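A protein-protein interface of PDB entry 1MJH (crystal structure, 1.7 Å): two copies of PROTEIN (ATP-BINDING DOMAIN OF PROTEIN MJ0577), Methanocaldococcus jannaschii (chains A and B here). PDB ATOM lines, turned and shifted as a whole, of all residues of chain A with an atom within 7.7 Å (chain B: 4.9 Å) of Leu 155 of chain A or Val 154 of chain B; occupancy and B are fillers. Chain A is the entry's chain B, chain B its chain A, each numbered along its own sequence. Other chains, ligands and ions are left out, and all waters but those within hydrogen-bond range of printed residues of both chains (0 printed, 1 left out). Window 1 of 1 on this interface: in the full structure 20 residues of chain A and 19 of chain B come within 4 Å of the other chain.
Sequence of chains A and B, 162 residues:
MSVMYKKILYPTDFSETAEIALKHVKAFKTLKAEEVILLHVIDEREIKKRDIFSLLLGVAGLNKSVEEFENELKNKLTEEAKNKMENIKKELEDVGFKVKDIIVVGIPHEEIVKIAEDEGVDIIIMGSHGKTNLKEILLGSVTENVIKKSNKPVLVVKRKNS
The side-chain hydroxyl (OH) of Tyr 5 of chain B lies within hydrogen-bond range of a ring nitrogen (ND1) of His 24 of chain A.
The side-chain amino group of Lys 158 of chain A sits at hydrogen-bond distance from the backbone carbonyl oxygen of Ile 147 of chain B (2.8 Å).
The backbone carbonyl oxygen of Val 154 of chain B sits at hydrogen-bond distance from the backbone NH of Val 156 of chain A (2.8 Å).
The backbone NH (N) of Val 156 of chain B sits at hydrogen-bond distance from the backbone carbonyl oxygen (O) of Val 154 of chain A (2.8 Å).
The backbone carbonyl oxygen of Val 154 of chain A lies close to the backbone carbonyl oxygen of Val 154 of chain B (3.3 Å).
The backbone NH (N) of Ile 124 of chain B is in hydrogen-bond range of the backbone carbonyl oxygen (O) of Pro 153 of chain B, 3.0 Å away.
The backbone NH (N) of Met 126 of chain B is in hydrogen-bond range of the backbone carbonyl oxygen (O) of Leu 155 of chain B, 3.0 Å away.
The backbone carbonyl oxygen (O) of Ile 123 of chain A lies within hydrogen-bond range of the backbone NH (N) of Leu 9 of chain A, at 2.9 Å.
The backbone NH (N) of Ile 124 of chain A lies within hydrogen-bond range of the backbone carbonyl oxygen (O) of Pro 153 of chain A (2.9 Å).
N of Leu 155 of chain A is in hydrogen-bond range of O of Ile 124 of chain A (2.8 Å).
O of Leu 155 of chain A is in hydrogen-bond range of N of Met 126 of chain A.
Ala 27 of chain A touches Tyr 5 of chain B.
CE1 of Phe 28 of chain A touches OH of Tyr 5 of chain B, 3.6 Å away.
CD1 of Leu 155 of chain B touches CD1 of Ile 123 of chain A (3.8 Å).
Pro 153 of chain A touches Leu 155 of chain B (CB to CD1, 3.99 Å).
Val 156 of chain B touches Pro 153 of chain A (O to CA, 3.3 Å).
Val 154 of chain A touches Leu 155 of chain B.
Tyr 5 of chain B touches Leu 155 of chain A (OH to CD2, 3.8 Å).
Leu 155 of chain A touches Leu 155 of chain B (N to CD1, 3.8 Å).
Val 156 of chain A touches Pro 153 of chain B.
CG of Lys 158 of chain A touches O of Lys 152 of chain B, at 3.5 Å.
Thr 143 of chain A touches none of the printed residues of chain B.
Printed residues of chain B within 4 Å of Leu 155 of chain A: Tyr 5 (3.8 Å), Ile 123 (3.8 Å), Pro 153 (3.995 Å), Val 154 (3.5 Å) and Leu 155 (3.8 Å).
Printed residues of chain A within 4 Å of Tyr 5 of chain B: His 24 (2.7 Å), Ala 27 (3.9 Å), Phe 28 (3.6 Å) and Leu 155 (3.8 Å).
Met 126 of chain B touches none of the printed residues of chain A.
Of the printed residues of chain A, Lys 152 of chain B touches Lys 158.
Of chain A, only Val 154 (3.3 Å), Leu 155 (3.5 Å) and Val 156 (2.8 Å) come within 4 Å of Val 154 of chain B.
The nearest printed residue of chain B that does not touch Leu 155 of chain A is Val 156 of chain B (4.8 Å).
The nearest residue of chain A that does not touch Val 154 of chain B is Val 157 of chain A (5.3 Å).
Hydrophobic or aromatic side chains of chain A within 4 Å of the printed part of chain B: His 24, Ala 27, Phe 28, Ile 123, Pro 153, Leu 155 and Val 156.
Ile 123 of chain A touches Leu 155 of chain B, and with the chains exchanged Leu 155 of chain A touches Ile 123 of chain B.
Pro 153 of chain A touches Val 156 of chain B, and with the chains exchanged Val 156 of chain A touches Pro 153 of chain B.
Val 154 of chain A touches its own counterpart, Val 154 of chain B.
Val 154 of chain A touches Val 156 of chain B, and with the chains exchanged Val 156 of chain A touches Val 154 of chain B.
Positions printed for both chains: 123, 124, 126, 147, 152, 153, 154, 155 and 156.
Of the 19 pairs that touch across the chains among the printed residues, 12 have their exchanged pair printed and touching as well.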
ATOM      1  N   LEU A   9      10.643  18.367 -28.933  1.00  0.00           N
ATOM      2  CA  LEU A   9      11.814  19.233 -29.147  1.00  0.00           C
ATOM      3  C   LEU A   9      12.211  19.766 -27.770  1.00  0.00           C
ATOM      4  O   LEU A   9      11.343  20.355 -27.107  1.00  0.00           O
ATOM      5  CB  LEU A   9      11.604  20.440 -30.066  1.00  0.00           C
ATOM      6  CG  LEU A   9      12.745  21.458 -30.220  1.00  0.00           C
ATOM      7  CD1 LEU A   9      14.005  20.771 -30.804  1.00  0.00           C
ATOM      8  CD2 LEU A   9      12.390  22.635 -31.126  1.00  0.00           C
ATOM      9  N   PRO A  11      14.929  22.241 -26.452  1.00  0.00           N
ATOM     10  CA  PRO A  11      16.018  23.180 -26.684  1.00  0.00           C
ATOM     11  C   PRO A  11      16.595  23.591 -25.324  1.00  0.00           C
ATOM     12  O   PRO A  11      15.849  23.989 -24.436  1.00  0.00           O
ATOM     13  CB  PRO A  11      15.323  24.371 -27.335  1.00  0.00           C
ATOM     14  CG  PRO A  11      13.895  24.355 -26.850  1.00  0.00           C
ATOM     15  CD  PRO A  11      13.618  22.948 -26.387  1.00  0.00           C
ATOM     16  N   ALA A  21      13.238  21.980 -16.870  1.00  0.00           N
ATOM     17  CA  ALA A  21      12.461  21.496 -18.042  1.00  0.00           C
ATOM     18  C   ALA A  21      12.864  20.102 -18.432  1.00  0.00           C
ATOM     19  O   ALA A  21      12.031  19.366 -18.975  1.00  0.00           O
ATOM     20  CB  ALA A  21      12.691  22.465 -19.219  1.00  0.00           C
ATOM     21  N   HIS A  24      10.626  17.526 -16.972  1.00  0.00           N
ATOM     22  CA  HIS A  24       9.325  17.386 -17.656  1.00  0.00           C
ATOM     23  C   HIS A  24       9.487  16.591 -18.931  1.00  0.00           C
ATOM     24  O   HIS A  24       8.627  15.740 -19.209  1.00  0.00           O
ATOM     25  CB  HIS A  24       8.712  18.776 -17.965  1.00  0.00           C
ATOM     26  CG  HIS A  24       8.355  19.448 -16.662  1.00  0.00           C
ATOM     27  ND1 HIS A  24       7.028  19.492 -16.251  1.00  0.00           N
ATOM     28  CD2 HIS A  24       9.117  20.094 -15.745  1.00  0.00           C
ATOM     29  CE1 HIS A  24       7.011  20.120 -15.075  1.00  0.00           C
ATOM     30  NE2 HIS A  24       8.261  20.498 -14.704  1.00  0.00           N
ATOM     31  N   VAL A  25      10.587  16.748 -19.665  1.00  0.00           N
ATOM     32  CA  VAL A  25      10.801  15.855 -20.819  1.00  0.00           C
ATOM     33  C   VAL A  25      10.778  14.392 -20.385  1.00  0.00           C
ATOM     34  O   VAL A  25      10.181  13.522 -21.046  1.00  0.00           O
ATOM     35  CB  VAL A  25      12.144  16.170 -21.500  1.00  0.00           C
ATOM     36  CG1 VAL A  25      12.416  15.218 -22.688  1.00  0.00           C
ATOM     37  CG2 VAL A  25      12.112  17.626 -22.013  1.00  0.00           C
ATOM     38  N   ALA A  27       9.259  13.149 -17.818  1.00  0.00           N
ATOM     39  CA  ALA A  27       7.913  12.756 -17.454  1.00  0.00           C
ATOM     40  C   ALA A  27       7.008  12.402 -18.598  1.00  0.00           C
ATOM     41  O   ALA A  27       5.968  11.737 -18.411  1.00  0.00           O
ATOM     42  CB  ALA A  27       7.302  13.839 -16.532  1.00  0.00           C
ATOM     43  N   PHE A  28       7.339  12.863 -19.818  1.00  0.00           N
ATOM     44  CA  PHE A  28       6.530  12.520 -20.987  1.00  0.00           C
ATOM     45  C   PHE A  28       6.790  11.077 -21.437  1.00  0.00           C
ATOM     46  O   PHE A  28       6.121  10.663 -22.359  1.00  0.00           O
ATOM     47  CB  PHE A  28       6.807  13.503 -22.118  1.00  0.00           C
ATOM     48  CG  PHE A  28       5.901  14.695 -22.134  1.00  0.00           C
ATOM     49  CD1 PHE A  28       5.884  15.592 -21.088  1.00  0.00           C
ATOM     50  CD2 PHE A  28       5.013  14.921 -23.185  1.00  0.00           C
ATOM     51  CE1 PHE A  28       5.047  16.689 -21.085  1.00  0.00           C
ATOM     52  CE2 PHE A  28       4.173  16.007 -23.175  1.00  0.00           C
ATOM     53  CZ  PHE A  28       4.174  16.896 -22.125  1.00  0.00           C
ATOM     54  N   ILE A 123       5.564  18.668 -29.758  1.00  0.00           N
ATOM     55  CA  ILE A 123       5.525  19.610 -28.618  1.00  0.00           C
ATOM     56  C   ILE A 123       6.943  20.125 -28.431  1.00  0.00           C
ATOM     57  O   ILE A 123       7.904  19.407 -28.772  1.00  0.00           O
ATOM     58  CB  ILE A 123       5.013  18.892 -27.367  1.00  0.00           C
ATOM     59  CG1 ILE A 123       4.966  19.889 -26.190  1.00  0.00           C
ATOM     60  CG2 ILE A 123       5.868  17.672 -26.978  1.00  0.00           C
ATOM     61  CD1 ILE A 123       4.217  19.281 -24.991  1.00  0.00           C
ATOM     62  N   ILE A 124       7.079  21.343 -27.959  1.00  0.00           N
ATOM     63  CA  ILE A 124       8.359  21.901 -27.566  1.00  0.00           C
ATOM     64  C   ILE A 124       8.326  22.029 -26.034  1.00  0.00           C
ATOM     65  O   ILE A 124       7.344  22.600 -25.546  1.00  0.00           O
ATOM     66  CB  ILE A 124       8.540  23.318 -28.143  1.00  0.00           C
ATOM     67  CG1 ILE A 124       8.400  23.210 -29.714  1.00  0.00           C
ATOM     68  CG2 ILE A 124       9.957  23.743 -27.827  1.00  0.00           C
ATOM     69  CD1 ILE A 124       8.557  24.557 -30.355  1.00  0.00           C
ATOM     70  N   ILE A 125       9.299  21.484 -25.320  1.00  0.00           N
ATOM     71  CA  ILE A 125       9.300  21.608 -23.826  1.00  0.00           C
ATOM     72  C   ILE A 125      10.529  22.476 -23.463  1.00  0.00           C
ATOM     73  O   ILE A 125      11.661  22.113 -23.783  1.00  0.00           O
ATOM     74  CB  ILE A 125       9.386  20.212 -23.207  1.00  0.00           C
ATOM     75  CG1 ILE A 125       8.102  19.409 -23.490  1.00  0.00           C
ATOM     76  CG2 ILE A 125       9.526  20.380 -21.670  1.00  0.00           C
ATOM     77  CD1 ILE A 125       8.101  17.999 -22.889  1.00  0.00           C
ATOM     78  N   MET A 126      10.332  23.630 -22.825  1.00  0.00           N
ATOM     79  CA  MET A 126      11.469  24.578 -22.629  1.00  0.00           C
ATOM     80  C   MET A 126      11.300  25.310 -21.310  1.00  0.00           C
ATOM     81  O   MET A 126      10.184  25.333 -20.778  1.00  0.00           O
ATOM     82  CB  MET A 126      11.642  25.533 -23.864  1.00  0.00           C
ATOM     83  CG  MET A 126      10.447  26.538 -24.008  1.00  0.00           C
ATOM     84  SD  MET A 126      10.350  27.345 -25.727  1.00  0.00           S
ATOM     85  CE  MET A 126      12.004  28.068 -25.700  1.00  0.00           C
ATOM     86  N   GLY A 127      12.388  25.979 -20.863  1.00  0.00           N
ATOM     87  CA  GLY A 127      12.218  26.759 -19.623  1.00  0.00           C
ATOM     88  C   GLY A 127      11.580  28.106 -19.917  1.00  0.00           C
ATOM     89  O   GLY A 127      11.558  28.602 -21.047  1.00  0.00           O
ATOM     90  N   SER A 128      11.057  28.742 -18.832  1.00  0.00           N
ATOM     91  CA  SER A 128      10.565  30.113 -18.952  1.00  0.00           C
ATOM     92  C   SER A 128      11.712  31.127 -19.029  1.00  0.00           C
ATOM     93  O   SER A 128      11.552  32.242 -19.554  1.00  0.00           O
ATOM     94  CB  SER A 128       9.694  30.477 -17.755  1.00  0.00           C
ATOM     95  OG  SER A 128      10.470  30.409 -16.553  1.00  0.00           O
ATOM     96  N   THR A 143      11.831  32.138 -25.160  1.00  0.00           N
ATOM     97  CA  THR A 143      10.523  31.504 -24.989  1.00  0.00           C
ATOM     98  C   THR A 143       9.383  32.365 -25.504  1.00  0.00           C
ATOM     99  O   THR A 143       8.499  31.835 -26.177  1.00  0.00           O
ATOM    100  CB  THR A 143      10.233  31.145 -23.506  1.00  0.00           C
ATOM    101  OG1 THR A 143      11.395  30.375 -23.130  1.00  0.00           O
ATOM    102  CG2 THR A 143       8.937  30.383 -23.394  1.00  0.00           C
ATOM    103  N   ILE A 147       6.929  30.968 -28.485  1.00  0.00           N
ATOM    104  CA  ILE A 147       5.481  30.782 -28.375  1.00  0.00           C
ATOM    105  C   ILE A 147       4.752  31.584 -29.467  1.00  0.00           C
ATOM    106  O   ILE A 147       3.739  31.118 -30.007  1.00  0.00           O
ATOM    107  CB  ILE A 147       5.012  31.261 -26.975  1.00  0.00           C
ATOM    108  CG1 ILE A 147       5.515  30.254 -25.904  1.00  0.00           C
ATOM    109  CG2 ILE A 147       3.507  31.421 -26.926  1.00  0.00           C
ATOM    110  CD1 ILE A 147       5.352  30.947 -24.535  1.00  0.00           C
ATOM    111  N   LYS A 152       3.632  25.151 -32.849  1.00  0.00           N
ATOM    112  CA  LYS A 152       3.644  23.926 -32.083  1.00  0.00           C
ATOM    113  C   LYS A 152       3.179  24.191 -30.648  1.00  0.00           C
ATOM    114  O   LYS A 152       3.455  25.314 -30.201  1.00  0.00           O
ATOM    115  CB  LYS A 152       5.098  23.402 -31.963  1.00  0.00           C
ATOM    116  CG  LYS A 152       5.691  22.964 -33.341  1.00  0.00           C
ATOM    117  CD  LYS A 152       4.924  21.859 -34.018  1.00  0.00           C
ATOM    118  CE  LYS A 152       5.671  21.494 -35.338  1.00  0.00           C
ATOM    119  NZ  LYS A 152       4.855  20.403 -35.988  1.00  0.00           N
ATOM    120  N   PRO A 153       2.662  23.201 -29.959  1.00  0.00           N
ATOM    121  CA  PRO A 153       2.356  23.345 -28.527  1.00  0.00           C
ATOM    122  C   PRO A 153       3.670  23.567 -27.774  1.00  0.00           C
ATOM    123  O   PRO A 153       4.692  22.932 -28.130  1.00  0.00           O
ATOM    124  CB  PRO A 153       1.727  22.003 -28.127  1.00  0.00           C
ATOM    125  CG  PRO A 153       1.301  21.345 -29.434  1.00  0.00           C
ATOM    126  CD  PRO A 153       2.281  21.869 -30.417  1.00  0.00           C
ATOM    127  N   VAL A 154       3.656  24.530 -26.844  1.00  0.00           N
ATOM    128  CA  VAL A 154       4.871  24.788 -26.045  1.00  0.00           C
ATOM    129  C   VAL A 154       4.578  24.618 -24.546  1.00  0.00           C
ATOM    130  O   VAL A 154       3.689  25.298 -24.014  1.00  0.00           O
ATOM    131  CB  VAL A 154       5.323  26.236 -26.261  1.00  0.00           C
ATOM    132  CG1 VAL A 154       6.619  26.506 -25.439  1.00  0.00           C
ATOM    133  CG2 VAL A 154       5.707  26.515 -27.726  1.00  0.00           C
ATOM    134  N   LEU A 155       5.293  23.676 -23.953  1.00  0.00           N
ATOM    135  CA  LEU A 155       5.224  23.516 -22.465  1.00  0.00           C
ATOM    136  C   LEU A 155       6.276  24.445 -21.887  1.00  0.00           C
ATOM    137  O   LEU A 155       7.456  24.192 -22.068  1.00  0.00           O
ATOM    138  CB  LEU A 155       5.416  22.055 -22.069  1.00  0.00           C
ATOM    139  CG  LEU A 155       5.513  21.822 -20.522  1.00  0.00           C
ATOM    140  CD1 LEU A 155       4.264  22.345 -19.832  1.00  0.00           C
ATOM    141  CD2 LEU A 155       5.644  20.300 -20.237  1.00  0.00           C
ATOM    142  N   VAL A 156       5.881  25.468 -21.135  1.00  0.00           N
ATOM    143  CA  VAL A 156       6.769  26.412 -20.511  1.00  0.00           C
ATOM    144  C   VAL A 156       6.950  26.032 -19.035  1.00  0.00           C
ATOM    145  O   VAL A 156       5.988  26.012 -18.289  1.00  0.00           O
ATOM    146  CB  VAL A 156       6.189  27.841 -20.541  1.00  0.00           C
ATOM    147  CG1 VAL A 156       7.216  28.778 -19.896  1.00  0.00           C
ATOM    148  CG2 VAL A 156       5.842  28.323 -21.968  1.00  0.00           C
ATOM    149  N   VAL A 157       8.172  25.624 -18.678  1.00  0.00           N
ATOM    150  CA  VAL A 157       8.458  25.184 -17.320  1.00  0.00           C
ATOM    151  C   VAL A 157       9.076  26.373 -16.568  1.00  0.00           C
ATOM    152  O   VAL A 157      10.089  26.904 -17.044  1.00  0.00           O
ATOM    153  CB  VAL A 157       9.465  24.035 -17.359  1.00  0.00           C
ATOM    154  CG1 VAL A 157       9.824  23.542 -15.940  1.00  0.00           C
ATOM    155  CG2 VAL A 157       8.870  22.807 -18.089  1.00  0.00           C
ATOM    156  N   LYS A 158       8.495  26.741 -15.440  1.00  0.00           N
ATOM    157  CA  LYS A 158       8.967  28.012 -14.831  1.00  0.00           C
ATOM    158  C   LYS A 158      10.247  27.842 -14.033  1.00  0.00           C
ATOM    159  O   LYS A 158      10.613  26.781 -13.528  1.00  0.00           O
ATOM    160  CB  LYS A 158       7.907  28.567 -13.836  1.00  0.00           C
ATOM    161  CG  LYS A 158       6.521  28.747 -14.490  1.00  0.00           C
ATOM    162  CD  LYS A 158       6.516  29.731 -15.612  1.00  0.00           C
ATOM    163  CE  LYS A 158       7.164  31.111 -15.428  1.00  0.00           C
ATOM    164  NZ  LYS A 158       6.391  31.927 -14.388  1.00  0.00           N
ATOM    165  N   TYR B   5       2.070  14.395 -13.772  1.00  0.00           N
ATOM    166  CA  TYR B   5       0.887  15.182 -14.089  1.00  0.00           C
ATOM    167  C   TYR B   5      -0.398  14.521 -13.599  1.00  0.00           C
ATOM    168  O   TYR B   5      -1.146  13.973 -14.404  1.00  0.00           O
ATOM    169  CB  TYR B   5       0.839  15.361 -15.624  1.00  0.00           C
ATOM    170  CG  TYR B   5       2.124  15.962 -16.164  1.00  0.00           C
ATOM    171  CD1 TYR B   5       2.542  17.233 -15.778  1.00  0.00           C
ATOM    172  CD2 TYR B   5       2.937  15.253 -17.046  1.00  0.00           C
ATOM    173  CE1 TYR B   5       3.741  17.787 -16.243  1.00  0.00           C
ATOM    174  CE2 TYR B   5       4.117  15.816 -17.520  1.00  0.00           C
ATOM    175  CZ  TYR B   5       4.521  17.081 -17.117  1.00  0.00           C
ATOM    176  OH  TYR B   5       5.700  17.582 -17.630  1.00  0.00           O
ATOM    177  N   ILE B 123      -0.011  21.103 -13.649  1.00  0.00           N
ATOM    178  CA  ILE B 123       0.136  21.760 -14.947  1.00  0.00           C
ATOM    179  C   ILE B 123      -1.134  22.515 -15.315  1.00  0.00           C
ATOM    180  O   ILE B 123      -2.220  22.095 -14.893  1.00  0.00           O
ATOM    181  CB  ILE B 123       0.482  20.686 -16.017  1.00  0.00           C
ATOM    182  CG1 ILE B 123       0.711  21.362 -17.395  1.00  0.00           C
ATOM    183  CG2 ILE B 123      -0.673  19.674 -16.188  1.00  0.00           C
ATOM    184  CD1 ILE B 123       1.399  20.355 -18.348  1.00  0.00           C
ATOM    185  N   ILE B 124      -1.042  23.602 -16.062  1.00  0.00           N
ATOM    186  CA  ILE B 124      -2.132  24.356 -16.625  1.00  0.00           C
ATOM    187  C   ILE B 124      -2.073  24.128 -18.149  1.00  0.00           C
ATOM    188  O   ILE B 124      -1.018  24.395 -18.736  1.00  0.00           O
ATOM    189  CB  ILE B 124      -1.971  25.879 -16.393  1.00  0.00           C
ATOM    190  CG1 ILE B 124      -1.806  26.063 -14.857  1.00  0.00           C
ATOM    191  CG2 ILE B 124      -3.243  26.580 -16.881  1.00  0.00           C
ATOM    192  CD1 ILE B 124      -1.564  27.566 -14.596  1.00  0.00           C
ATOM    193  N   MET B 126      -3.812  25.290 -21.676  1.00  0.00           N
ATOM    194  CA  MET B 126      -4.715  26.362 -22.124  1.00  0.00           C
ATOM    195  C   MET B 126      -4.452  26.787 -23.560  1.00  0.00           C
ATOM    196  O   MET B 126      -3.376  26.499 -24.067  1.00  0.00           O
ATOM    197  CB  MET B 126      -4.623  27.601 -21.169  1.00  0.00           C
ATOM    198  CG  MET B 126      -3.248  28.365 -21.181  1.00  0.00           C
ATOM    199  SD  MET B 126      -2.940  29.511 -19.716  1.00  0.00           S
ATOM    200  CE  MET B 126      -4.399  30.576 -19.943  1.00  0.00           C
ATOM    201  N   VAL B 146      -0.979  34.581 -17.353  1.00  0.00           N
ATOM    202  CA  VAL B 146      -0.817  33.346 -16.515  1.00  0.00           C
ATOM    203  C   VAL B 146       0.591  32.831 -16.569  1.00  0.00           C
ATOM    204  O   VAL B 146       1.165  32.501 -15.521  1.00  0.00           O
ATOM    205  CB  VAL B 146      -1.812  32.246 -16.975  1.00  0.00           C
ATOM    206  CG1 VAL B 146      -1.551  30.887 -16.333  1.00  0.00           C
ATOM    207  CG2 VAL B 146      -3.231  32.805 -16.712  1.00  0.00           C
ATOM    208  N   ILE B 147       1.237  32.760 -17.758  1.00  0.00           N
ATOM    209  CA  ILE B 147       2.658  32.374 -17.828  1.00  0.00           C
ATOM    210  C   ILE B 147       3.553  33.264 -16.984  1.00  0.00           C
ATOM    211  O   ILE B 147       4.437  32.744 -16.280  1.00  0.00           O
ATOM    212  CB  ILE B 147       3.198  32.466 -19.295  1.00  0.00           C
ATOM    213  CG1 ILE B 147       2.388  31.407 -20.063  1.00  0.00           C
ATOM    214  CG2 ILE B 147       4.697  32.184 -19.272  1.00  0.00           C
ATOM    215  CD1 ILE B 147       2.637  31.621 -21.577  1.00  0.00           C
ATOM    216  N   LYS B 152       3.308  27.569 -12.070  1.00  0.00           N
ATOM    217  CA  LYS B 152       2.968  26.247 -12.575  1.00  0.00           C
ATOM    218  C   LYS B 152       3.421  26.124 -14.051  1.00  0.00           C
ATOM    219  O   LYS B 152       3.463  27.134 -14.774  1.00  0.00           O
ATOM    220  CB  LYS B 152       1.435  26.037 -12.616  1.00  0.00           C
ATOM    221  CG  LYS B 152       0.760  26.151 -11.240  1.00  0.00           C
ATOM    222  CD  LYS B 152       1.334  25.080 -10.315  1.00  0.00           C
ATOM    223  CE  LYS B 152       0.619  25.119  -8.968  1.00  0.00           C
ATOM    224  NZ  LYS B 152       1.079  24.048  -8.023  1.00  0.00           N
ATOM    225  N   PRO B 153       3.817  24.935 -14.449  1.00  0.00           N
ATOM    226  CA  PRO B 153       4.125  24.672 -15.865  1.00  0.00           C
ATOM    227  C   PRO B 153       2.853  24.973 -16.679  1.00  0.00           C
ATOM    228  O   PRO B 153       1.753  24.714 -16.225  1.00  0.00           O
ATOM    229  CB  PRO B 153       4.418  23.171 -15.926  1.00  0.00           C
ATOM    230  CG  PRO B 153       4.765  22.807 -14.495  1.00  0.00           C
ATOM    231  CD  PRO B 153       3.784  23.650 -13.663  1.00  0.00           C
ATOM    232  N   VAL B 154       2.981  25.587 -17.849  1.00  0.00           N
ATOM    233  CA  VAL B 154       1.834  25.924 -18.705  1.00  0.00           C
ATOM    234  C   VAL B 154       2.102  25.328 -20.088  1.00  0.00           C
ATOM    235  O   VAL B 154       3.068  25.699 -20.753  1.00  0.00           O
ATOM    236  CB  VAL B 154       1.604  27.431 -18.874  1.00  0.00           C
ATOM    237  CG1 VAL B 154       0.440  27.845 -19.780  1.00  0.00           C
ATOM    238  CG2 VAL B 154       1.306  28.081 -17.507  1.00  0.00           C
ATOM    239  N   LEU B 155       1.111  24.497 -20.509  1.00  0.00           N
ATOM    240  CA  LEU B 155       1.165  24.000 -21.898  1.00  0.00           C
ATOM    241  C   LEU B 155       0.279  24.933 -22.723  1.00  0.00           C
ATOM    242  O   LEU B 155      -0.922  25.048 -22.523  1.00  0.00           O
ATOM    243  CB  LEU B 155       0.618  22.555 -21.888  1.00  0.00           C
ATOM    244  CG  LEU B 155       0.512  21.950 -23.323  1.00  0.00           C
ATOM    245  CD1 LEU B 155       1.786  22.136 -24.135  1.00  0.00           C
ATOM    246  CD2 LEU B 155       0.156  20.459 -23.211  1.00  0.00           C
ATOM    247  N   VAL B 156       0.909  25.677 -23.610  1.00  0.00           N
ATOM    248  CA  VAL B 156       0.223  26.602 -24.515  1.00  0.00           C
ATOM    249  C   VAL B 156      -0.112  25.832 -25.806  1.00  0.00           C
ATOM    250  O   VAL B 156       0.790  25.457 -26.529  1.00  0.00           O
ATOM    251  CB  VAL B 156       1.099  27.801 -24.820  1.00  0.00           C
ATOM    252  CG1 VAL B 156       0.296  28.794 -25.697  1.00  0.00           C
ATOM    253  CG2 VAL B 156       1.491  28.500 -23.477  1.00  0.00           C
